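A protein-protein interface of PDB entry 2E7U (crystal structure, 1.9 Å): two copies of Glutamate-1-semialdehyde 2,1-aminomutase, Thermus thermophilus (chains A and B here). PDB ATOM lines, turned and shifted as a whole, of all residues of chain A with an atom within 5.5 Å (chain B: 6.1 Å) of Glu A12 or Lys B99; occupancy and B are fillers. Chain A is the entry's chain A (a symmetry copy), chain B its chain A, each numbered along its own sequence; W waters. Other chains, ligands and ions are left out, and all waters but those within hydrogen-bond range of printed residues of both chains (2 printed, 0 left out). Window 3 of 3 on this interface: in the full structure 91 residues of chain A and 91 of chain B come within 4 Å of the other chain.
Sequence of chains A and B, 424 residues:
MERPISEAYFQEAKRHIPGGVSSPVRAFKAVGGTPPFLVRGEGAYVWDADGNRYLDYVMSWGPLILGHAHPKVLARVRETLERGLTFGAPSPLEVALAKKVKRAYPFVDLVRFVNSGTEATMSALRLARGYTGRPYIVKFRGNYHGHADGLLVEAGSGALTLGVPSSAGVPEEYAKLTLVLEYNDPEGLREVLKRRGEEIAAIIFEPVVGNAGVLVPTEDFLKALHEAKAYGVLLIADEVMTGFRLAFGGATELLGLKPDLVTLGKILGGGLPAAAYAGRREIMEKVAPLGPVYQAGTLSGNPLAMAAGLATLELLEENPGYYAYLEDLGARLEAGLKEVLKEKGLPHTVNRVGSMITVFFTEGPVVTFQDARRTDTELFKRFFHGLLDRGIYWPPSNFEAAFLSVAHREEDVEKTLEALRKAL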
ATOM      1  N   GLU A   7     -21.834  12.496   2.701  1.00  0.00           N
ATOM      2  CA  GLU A   7     -20.742  11.529   2.704  1.00  0.00           C
ATOM      3  C   GLU A   7     -20.972  10.493   3.796  1.00  0.00           C
ATOM      4  O   GLU A   7     -20.774   9.294   3.580  1.00  0.00           O
ATOM      5  CB  GLU A   7     -19.403  12.240   2.926  1.00  0.00           C
ATOM      6  CG  GLU A   7     -18.878  12.944   1.683  1.00  0.00           C
ATOM      7  CD  GLU A   7     -17.700  13.863   1.977  1.00  0.00           C
ATOM      8  OE1 GLU A   7     -16.852  13.506   2.821  1.00  0.00           O
ATOM      9  OE2 GLU A   7     -17.619  14.940   1.352  1.00  0.00           O
ATOM     10  N   ALA A   8     -21.403  10.957   4.966  1.00  0.00           N
ATOM     11  CA  ALA A   8     -21.668  10.066   6.087  1.00  0.00           C
ATOM     12  C   ALA A   8     -22.861   9.167   5.760  1.00  0.00           C
ATOM     13  O   ALA A   8     -22.844   7.973   6.060  1.00  0.00           O
ATOM     14  CB  ALA A   8     -21.939  10.881   7.359  1.00  0.00           C
ATOM     15  N   TYR A   9     -23.896   9.738   5.149  1.00  0.00           N
ATOM     16  CA  TYR A   9     -25.067   8.950   4.780  1.00  0.00           C
ATOM     17  C   TYR A   9     -24.733   7.881   3.745  1.00  0.00           C
ATOM     18  O   TYR A   9     -25.232   6.757   3.822  1.00  0.00           O
ATOM     19  CB  TYR A   9     -26.177   9.846   4.222  1.00  0.00           C
ATOM     20  CG  TYR A   9     -27.150  10.328   5.272  1.00  0.00           C
ATOM     21  CD1 TYR A   9     -27.984   9.433   5.942  1.00  0.00           C
ATOM     22  CD2 TYR A   9     -27.236  11.678   5.598  1.00  0.00           C
ATOM     23  CE1 TYR A   9     -28.881   9.876   6.917  1.00  0.00           C
ATOM     24  CE2 TYR A   9     -28.127  12.129   6.564  1.00  0.00           C
ATOM     25  CZ  TYR A   9     -28.944  11.227   7.218  1.00  0.00           C
ATOM     26  OH  TYR A   9     -29.816  11.688   8.173  1.00  0.00           O
ATOM     27  N   PHE A  10     -23.895   8.229   2.775  1.00  0.00           N
ATOM     28  CA  PHE A  10     -23.521   7.279   1.734  1.00  0.00           C
ATOM     29  C   PHE A  10     -22.745   6.104   2.318  1.00  0.00           C
ATOM     30  O   PHE A  10     -22.958   4.952   1.933  1.00  0.00           O
ATOM     31  CB  PHE A  10     -22.692   7.982   0.656  1.00  0.00           C
ATOM     32  CG  PHE A  10     -22.576   7.204  -0.623  1.00  0.00           C
ATOM     33  CD1 PHE A  10     -23.701   6.626  -1.205  1.00  0.00           C
ATOM     34  CD2 PHE A  10     -21.349   7.078  -1.265  1.00  0.00           C
ATOM     35  CE1 PHE A  10     -23.607   5.934  -2.408  1.00  0.00           C
ATOM     36  CE2 PHE A  10     -21.246   6.387  -2.471  1.00  0.00           C
ATOM     37  CZ  PHE A  10     -22.378   5.815  -3.041  1.00  0.00           C
ATOM     38  N   GLN A  11     -21.840   6.394   3.248  1.00  0.00           N
ATOM     39  CA  GLN A  11     -21.056   5.341   3.884  1.00  0.00           C
ATOM     40  C   GLN A  11     -21.983   4.423   4.685  1.00  0.00           C
ATOM     41  O   GLN A  11     -21.828   3.200   4.672  1.00  0.00           O
ATOM     42  CB  GLN A  11     -19.992   5.953   4.803  1.00  0.00           C
ATOM     43  CG  GLN A  11     -19.194   4.936   5.610  1.00  0.00           C
ATOM     44  CD  GLN A  11     -18.148   5.586   6.501  1.00  0.00           C
ATOM     45  OE1 GLN A  11     -18.452   6.487   7.287  1.00  0.00           O
ATOM     46  NE2 GLN A  11     -16.906   5.129   6.386  1.00  0.00           N
ATOM     47  N   GLU A  12     -22.948   5.016   5.382  1.00  0.00           N
ATOM     48  CA  GLU A  12     -23.897   4.235   6.169  1.00  0.00           C
ATOM     49  C   GLU A  12     -24.824   3.438   5.246  1.00  0.00           C
ATOM     50  O   GLU A  12     -25.097   2.261   5.486  1.00  0.00           O
ATOM     51  CB  GLU A  12     -24.724   5.163   7.070  1.00  0.00           C
ATOM     52  CG  GLU A  12     -25.806   4.469   7.895  1.00  0.00           C
ATOM     53  CD  GLU A  12     -25.255   3.548   8.979  1.00  0.00           C
ATOM     54  OE1 GLU A  12     -24.016   3.418   9.102  1.00  0.00           O
ATOM     55  OE2 GLU A  12     -26.075   2.954   9.714  1.00  0.00           O
ATOM     56  N   ALA A  13     -25.297   4.081   4.182  1.00  0.00           N
ATOM     57  CA  ALA A  13     -26.194   3.430   3.234  1.00  0.00           C
ATOM     58  C   ALA A  13     -25.592   2.146   2.660  1.00  0.00           C
ATOM     59  O   ALA A  13     -26.290   1.141   2.499  1.00  0.00           O
ATOM     60  CB  ALA A  13     -26.548   4.395   2.102  1.00  0.00           C
ATOM     61  N   LYS A  14     -24.297   2.181   2.359  1.00  0.00           N
ATOM     62  CA  LYS A  14     -23.606   1.022   1.791  1.00  0.00           C
ATOM     63  C   LYS A  14     -23.601  -0.197   2.708  1.00  0.00           C
ATOM     64  O   LYS A  14     -23.419  -1.325   2.251  1.00  0.00           O
ATOM     65  CB  LYS A  14     -22.163   1.389   1.434  1.00  0.00           C
ATOM     66  CG  LYS A  14     -22.035   2.317   0.245  1.00  0.00           C
ATOM     67  CD  LYS A  14     -20.581   2.674   0.001  1.00  0.00           C
ATOM     68  CE  LYS A  14     -20.414   3.485  -1.267  1.00  0.00           C
ATOM     69  NZ  LYS A  14     -18.987   3.872  -1.488  1.00  0.00           N
ATOM     70  N   ARG A  15     -23.798   0.028   4.000  1.00  0.00           N
ATOM     71  CA  ARG A  15     -23.818  -1.070   4.958  1.00  0.00           C
ATOM     72  C   ARG A  15     -25.160  -1.807   4.950  1.00  0.00           C
ATOM     73  O   ARG A  15     -25.248  -2.945   5.411  1.00  0.00           O
ATOM     74  CB  ARG A  15     -23.575  -0.544   6.376  1.00  0.00           C
ATOM     75  CG  ARG A  15     -22.279   0.238   6.576  1.00  0.00           C
ATOM     76  CD  ARG A  15     -22.231   0.796   7.997  1.00  0.00           C
ATOM     77  NE  ARG A  15     -22.272  -0.280   8.982  1.00  0.00           N
ATOM     78  CZ  ARG A  15     -22.826  -0.182  10.185  1.00  0.00           C
ATOM     79  NH1 ARG A  15     -23.398   0.954  10.572  1.00  0.00           N
ATOM     80  NH2 ARG A  15     -22.819  -1.228  11.002  1.00  0.00           N
ATOM     81  N   HIS A  16     -26.191  -1.164   4.409  1.00  0.00           N
ATOM     82  CA  HIS A  16     -27.538  -1.738   4.416  1.00  0.00           C
ATOM     83  C   HIS A  16     -28.220  -1.891   3.061  1.00  0.00           C
ATOM     84  O   HIS A  16     -29.239  -2.573   2.958  1.00  0.00           O
ATOM     85  CB  HIS A  16     -28.440  -0.874   5.306  1.00  0.00           C
ATOM     86  CG  HIS A  16     -27.791  -0.441   6.584  1.00  0.00           C
ATOM     87  ND1 HIS A  16     -27.362  -1.335   7.541  1.00  0.00           N
ATOM     88  CD2 HIS A  16     -27.482   0.792   7.055  1.00  0.00           C
ATOM     89  CE1 HIS A  16     -26.817  -0.674   8.547  1.00  0.00           C
ATOM     90  NE2 HIS A  16     -26.877   0.619   8.277  1.00  0.00           N
ATOM     91  N   GLU B  94     -34.604   5.983   2.906  1.00  0.00           N
ATOM     92  CA  GLU B  94     -34.323   4.636   2.407  1.00  0.00           C
ATOM     93  C   GLU B  94     -33.385   3.907   3.362  1.00  0.00           C
ATOM     94  O   GLU B  94     -33.577   2.728   3.663  1.00  0.00           O
ATOM     95  CB  GLU B  94     -33.673   4.705   1.022  1.00  0.00           C
ATOM     96  CG  GLU B  94     -34.600   5.180  -0.077  1.00  0.00           C
ATOM     97  CD  GLU B  94     -33.849   5.548  -1.345  1.00  0.00           C
ATOM     98  OE1 GLU B  94     -33.210   6.621  -1.371  1.00  0.00           O
ATOM     99  OE2 GLU B  94     -33.892   4.762  -2.311  1.00  0.00           O
ATOM    100  N   VAL B  95     -32.358   4.610   3.824  1.00  0.00           N
ATOM    101  CA  VAL B  95     -31.403   4.024   4.755  1.00  0.00           C
ATOM    102  C   VAL B  95     -32.120   3.628   6.047  1.00  0.00           C
ATOM    103  O   VAL B  95     -31.863   2.568   6.617  1.00  0.00           O
ATOM    104  CB  VAL B  95     -30.279   5.025   5.109  1.00  0.00           C
ATOM    105  CG1 VAL B  95     -29.298   4.381   6.085  1.00  0.00           C
ATOM    106  CG2 VAL B  95     -29.558   5.467   3.840  1.00  0.00           C
ATOM    107  N   ALA B  96     -33.023   4.486   6.506  1.00  0.00           N
ATOM    108  CA  ALA B  96     -33.757   4.216   7.736  1.00  0.00           C
ATOM    109  C   ALA B  96     -34.636   2.974   7.603  1.00  0.00           C
ATOM    110  O   ALA B  96     -34.658   2.123   8.496  1.00  0.00           O
ATOM    111  CB  ALA B  96     -34.609   5.425   8.114  1.00  0.00           C
ATOM    112  N   LEU B  97     -35.354   2.864   6.490  1.00  0.00           N
ATOM    113  CA  LEU B  97     -36.235   1.714   6.290  1.00  0.00           C
ATOM    114  C   LEU B  97     -35.431   0.426   6.120  1.00  0.00           C
ATOM    115  O   LEU B  97     -35.824  -0.629   6.618  1.00  0.00           O
ATOM    116  CB  LEU B  97     -37.152   1.936   5.080  1.00  0.00           C
ATOM    117  CG  LEU B  97     -38.268   0.890   4.914  1.00  0.00           C
ATOM    118  CD1 LEU B  97     -39.075   0.786   6.194  1.00  0.00           C
ATOM    119  CD2 LEU B  97     -39.181   1.278   3.749  1.00  0.00           C
ATOM    120  N   ALA B  98     -34.300   0.513   5.427  1.00  0.00           N
ATOM    121  CA  ALA B  98     -33.452  -0.658   5.230  1.00  0.00           C
ATOM    122  C   ALA B  98     -32.972  -1.177   6.586  1.00  0.00           C
ATOM    123  O   ALA B  98     -32.935  -2.387   6.818  1.00  0.00           O
ATOM    124  CB  ALA B  98     -32.259  -0.304   4.347  1.00  0.00           C
ATOM    125  N   LYS B  99     -32.600  -0.264   7.484  1.00  0.00           N
ATOM    126  CA  LYS B  99     -32.142  -0.665   8.813  1.00  0.00           C
ATOM    127  C   LYS B  99     -33.263  -1.347   9.593  1.00  0.00           C
ATOM    128  O   LYS B  99     -33.019  -2.303  10.328  1.00  0.00           O
ATOM    129  CB  LYS B  99     -31.622   0.550   9.597  1.00  0.00           C
ATOM    130  CG  LYS B  99     -30.293   1.083   9.080  1.00  0.00           C
ATOM    131  CD  LYS B  99     -29.844   2.317   9.859  1.00  0.00           C
ATOM    132  CE  LYS B  99     -29.692   2.020  11.341  1.00  0.00           C
ATOM    133  NZ  LYS B  99     -29.420   3.265  12.114  1.00  0.00           N
ATOM    134  N   LYS B 100     -34.490  -0.857   9.432  1.00  0.00           N
ATOM    135  CA  LYS B 100     -35.640  -1.446  10.113  1.00  0.00           C
ATOM    136  C   LYS B 100     -35.862  -2.868   9.616  1.00  0.00           C
ATOM    137  O   LYS B 100     -36.156  -3.768  10.400  1.00  0.00           O
ATOM    138  CB  LYS B 100     -36.905  -0.618   9.866  1.00  0.00           C
ATOM    139  CG  LYS B 100     -37.030   0.605  10.752  1.00  0.00           C
ATOM    140  CD  LYS B 100     -36.995   0.209  12.223  1.00  0.00           C
ATOM    141  CE  LYS B 100     -37.041   1.433  13.121  1.00  0.00           C
ATOM    142  NZ  LYS B 100     -36.614   1.093  14.502  1.00  0.00           N
ATOM    143  N   VAL B 101     -35.729  -3.063   8.307  1.00  0.00           N
ATOM    144  CA  VAL B 101     -35.893  -4.388   7.721  1.00  0.00           C
ATOM    145  C   VAL B 101     -34.851  -5.331   8.330  1.00  0.00           C
ATOM    146  O   VAL B 101     -35.153  -6.476   8.671  1.00  0.00           O
ATOM    147  CB  VAL B 101     -35.708  -4.351   6.184  1.00  0.00           C
ATOM    148  CG1 VAL B 101     -35.672  -5.773   5.627  1.00  0.00           C
ATOM    149  CG2 VAL B 101     -36.850  -3.569   5.537  1.00  0.00           C
ATOM    150  N   LYS B 102     -33.626  -4.837   8.478  1.00  0.00           N
ATOM    151  CA  LYS B 102     -32.547  -5.637   9.039  1.00  0.00           C
ATOM    152  C   LYS B 102     -32.762  -5.987  10.511  1.00  0.00           C
ATOM    153  O   LYS B 102     -32.205  -6.965  11.003  1.00  0.00           O
ATOM    154  CB  LYS B 102     -31.200  -4.928   8.826  1.00  0.00           C
ATOM    155  CG  LYS B 102     -30.765  -4.928   7.356  1.00  0.00           C
ATOM    156  CD  LYS B 102     -29.469  -4.165   7.103  1.00  0.00           C
ATOM    157  CE  LYS B 102     -28.304  -4.748   7.891  1.00  0.00           C
ATOM    158  NZ  LYS B 102     -27.000  -4.167   7.453  1.00  0.00           N
ATOM    159  N   ARG B 103     -33.575  -5.202  11.213  1.00  0.00           N
ATOM    160  CA  ARG B 103     -33.862  -5.500  12.614  1.00  0.00           C
ATOM    161  C   ARG B 103     -34.879  -6.641  12.660  1.00  0.00           C
ATOM    162  O   ARG B 103     -34.836  -7.500  13.541  1.00  0.00           O
ATOM    163  CB  ARG B 103     -34.421  -4.262  13.320  1.00  0.00           C
ATOM    164  CG  ARG B 103     -33.372  -3.181  13.536  1.00  0.00           C
ATOM    165  CD  ARG B 103     -33.997  -1.809  13.716  1.00  0.00           C
ATOM    166  NE  ARG B 103     -34.545  -1.588  15.050  1.00  0.00           N
ATOM    167  CZ  ARG B 103     -33.808  -1.440  16.145  1.00  0.00           C
ATOM    168  NH1 ARG B 103     -32.483  -1.491  16.069  1.00  0.00           N
ATOM    169  NH2 ARG B 103     -34.394  -1.225  17.316  1.00  0.00           N
ATOM    170  N   ALA B 104     -35.785  -6.646  11.687  1.00  0.00           N
ATOM    171  CA  ALA B 104     -36.817  -7.672  11.594  1.00  0.00           C
ATOM    172  C   ALA B 104     -36.238  -8.973  11.038  1.00  0.00           C
ATOM    173  O   ALA B 104     -36.704 -10.065  11.374  1.00  0.00           O
ATOM    174  CB  ALA B 104     -37.944  -7.183  10.699  1.00  0.00           C
ATOM    175  N   VAL B 111     -30.379  -4.688   1.636  1.00  0.00           N
ATOM    176  CA  VAL B 111     -31.767  -4.579   1.205  1.00  0.00           C
ATOM    177  C   VAL B 111     -31.890  -3.694  -0.033  1.00  0.00           C
ATOM    178  O   VAL B 111     -31.362  -2.580  -0.056  1.00  0.00           O
ATOM    179  CB  VAL B 111     -32.633  -3.942   2.323  1.00  0.00           C
ATOM    180  CG1 VAL B 111     -34.086  -3.869   1.889  1.00  0.00           C
ATOM    181  CG2 VAL B 111     -32.484  -4.733   3.615  1.00  0.00           C
HETATM  182  O   HOH W   1     -26.331   2.059  12.271  1.00  0.00           O
HETATM  183  O   HOH W   2     -27.985   5.132  10.772  1.00  0.00           O
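Of the 10 printed residues of chain A, 4 touch a printed residue of chain B. Hydrophobic or aromatic side chains of chain A within 4 Å of the printed part of chain B: Ala A13 and His A16. Of the 12 printed residues of chain B, 5 touch a printed residue of chain A. Printed residues of chain B that touch a printed residue of chain A: Val B95, Ala B98, Lys B99, Lys B102 and Val B111. Along chain B the printed residues that touch a printed residue of chain A span positions 95 to 111. Among the printed residues, no Asp or Glu carboxylate lies within 4 Å of a Lys or Arg side-chain nitrogen of the other chain.
Among the printed residues, pairs that only touch across the chains: His A16 with Lys B99, Ala A13 with Val B95, Glu A12 with Lys B99, Glu A12 with Val B95 and His A16 with Ala B98.
No position is printed for both chains. Of the 8 pairs that touch across the chains among the printed residues, none has its exchanged pair printed and touching as well.
The side-chain amino group (NZ) of Lys B102 sits at hydrogen-bond distance from a ring nitrogen (ND1) of His A16 (2.9 Å). The backbone NH (N) of Val B111 sits at hydrogen-bond distance from the backbone carbonyl oxygen (O) of His A16 (2.7 Å). NZ of Lys B102 is in hydrogen-bond range of O of Arg A15, 3.0 Å away.
Water W2 lies within hydrogen-bond range of the side-chain amino group of Lys B99 (2.7 Å) and the side-chain carboxylate of Glu A12 (3.1 Å). Water W1 bridges the side-chain carboxylate of Glu A12 (2.7 Å) and the side-chain amino group of Lys B99 (3.3 Å).
The side-chain carboxylate (OE2) of Glu A12 lies within hydrogen-bond range of a ring nitrogen (NE2) of His A16 (2.9 Å). OE1 of Glu A12 is in salt-bridge range of NH1 of Arg A15, 2.9 Å away.
Of chain B, only Val B95 and Lys B99 come within 4 Å of Glu A12. Of the printed residues of chain B, Arg A15 touches Lys B102. Printed residues of chain B within 4 Å of Ala A13: Val B95. Printed residues of chain A within 4 Å of Val B95: Glu A12 (3.9 Å) and Ala A13 (3.6 Å). Of the printed residues of chain A, Ala B98 touches His A16 (3.98 Å). The nearest printed residue of chain B that does not touch Glu A12 is Lys B102 (7.0 Å).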
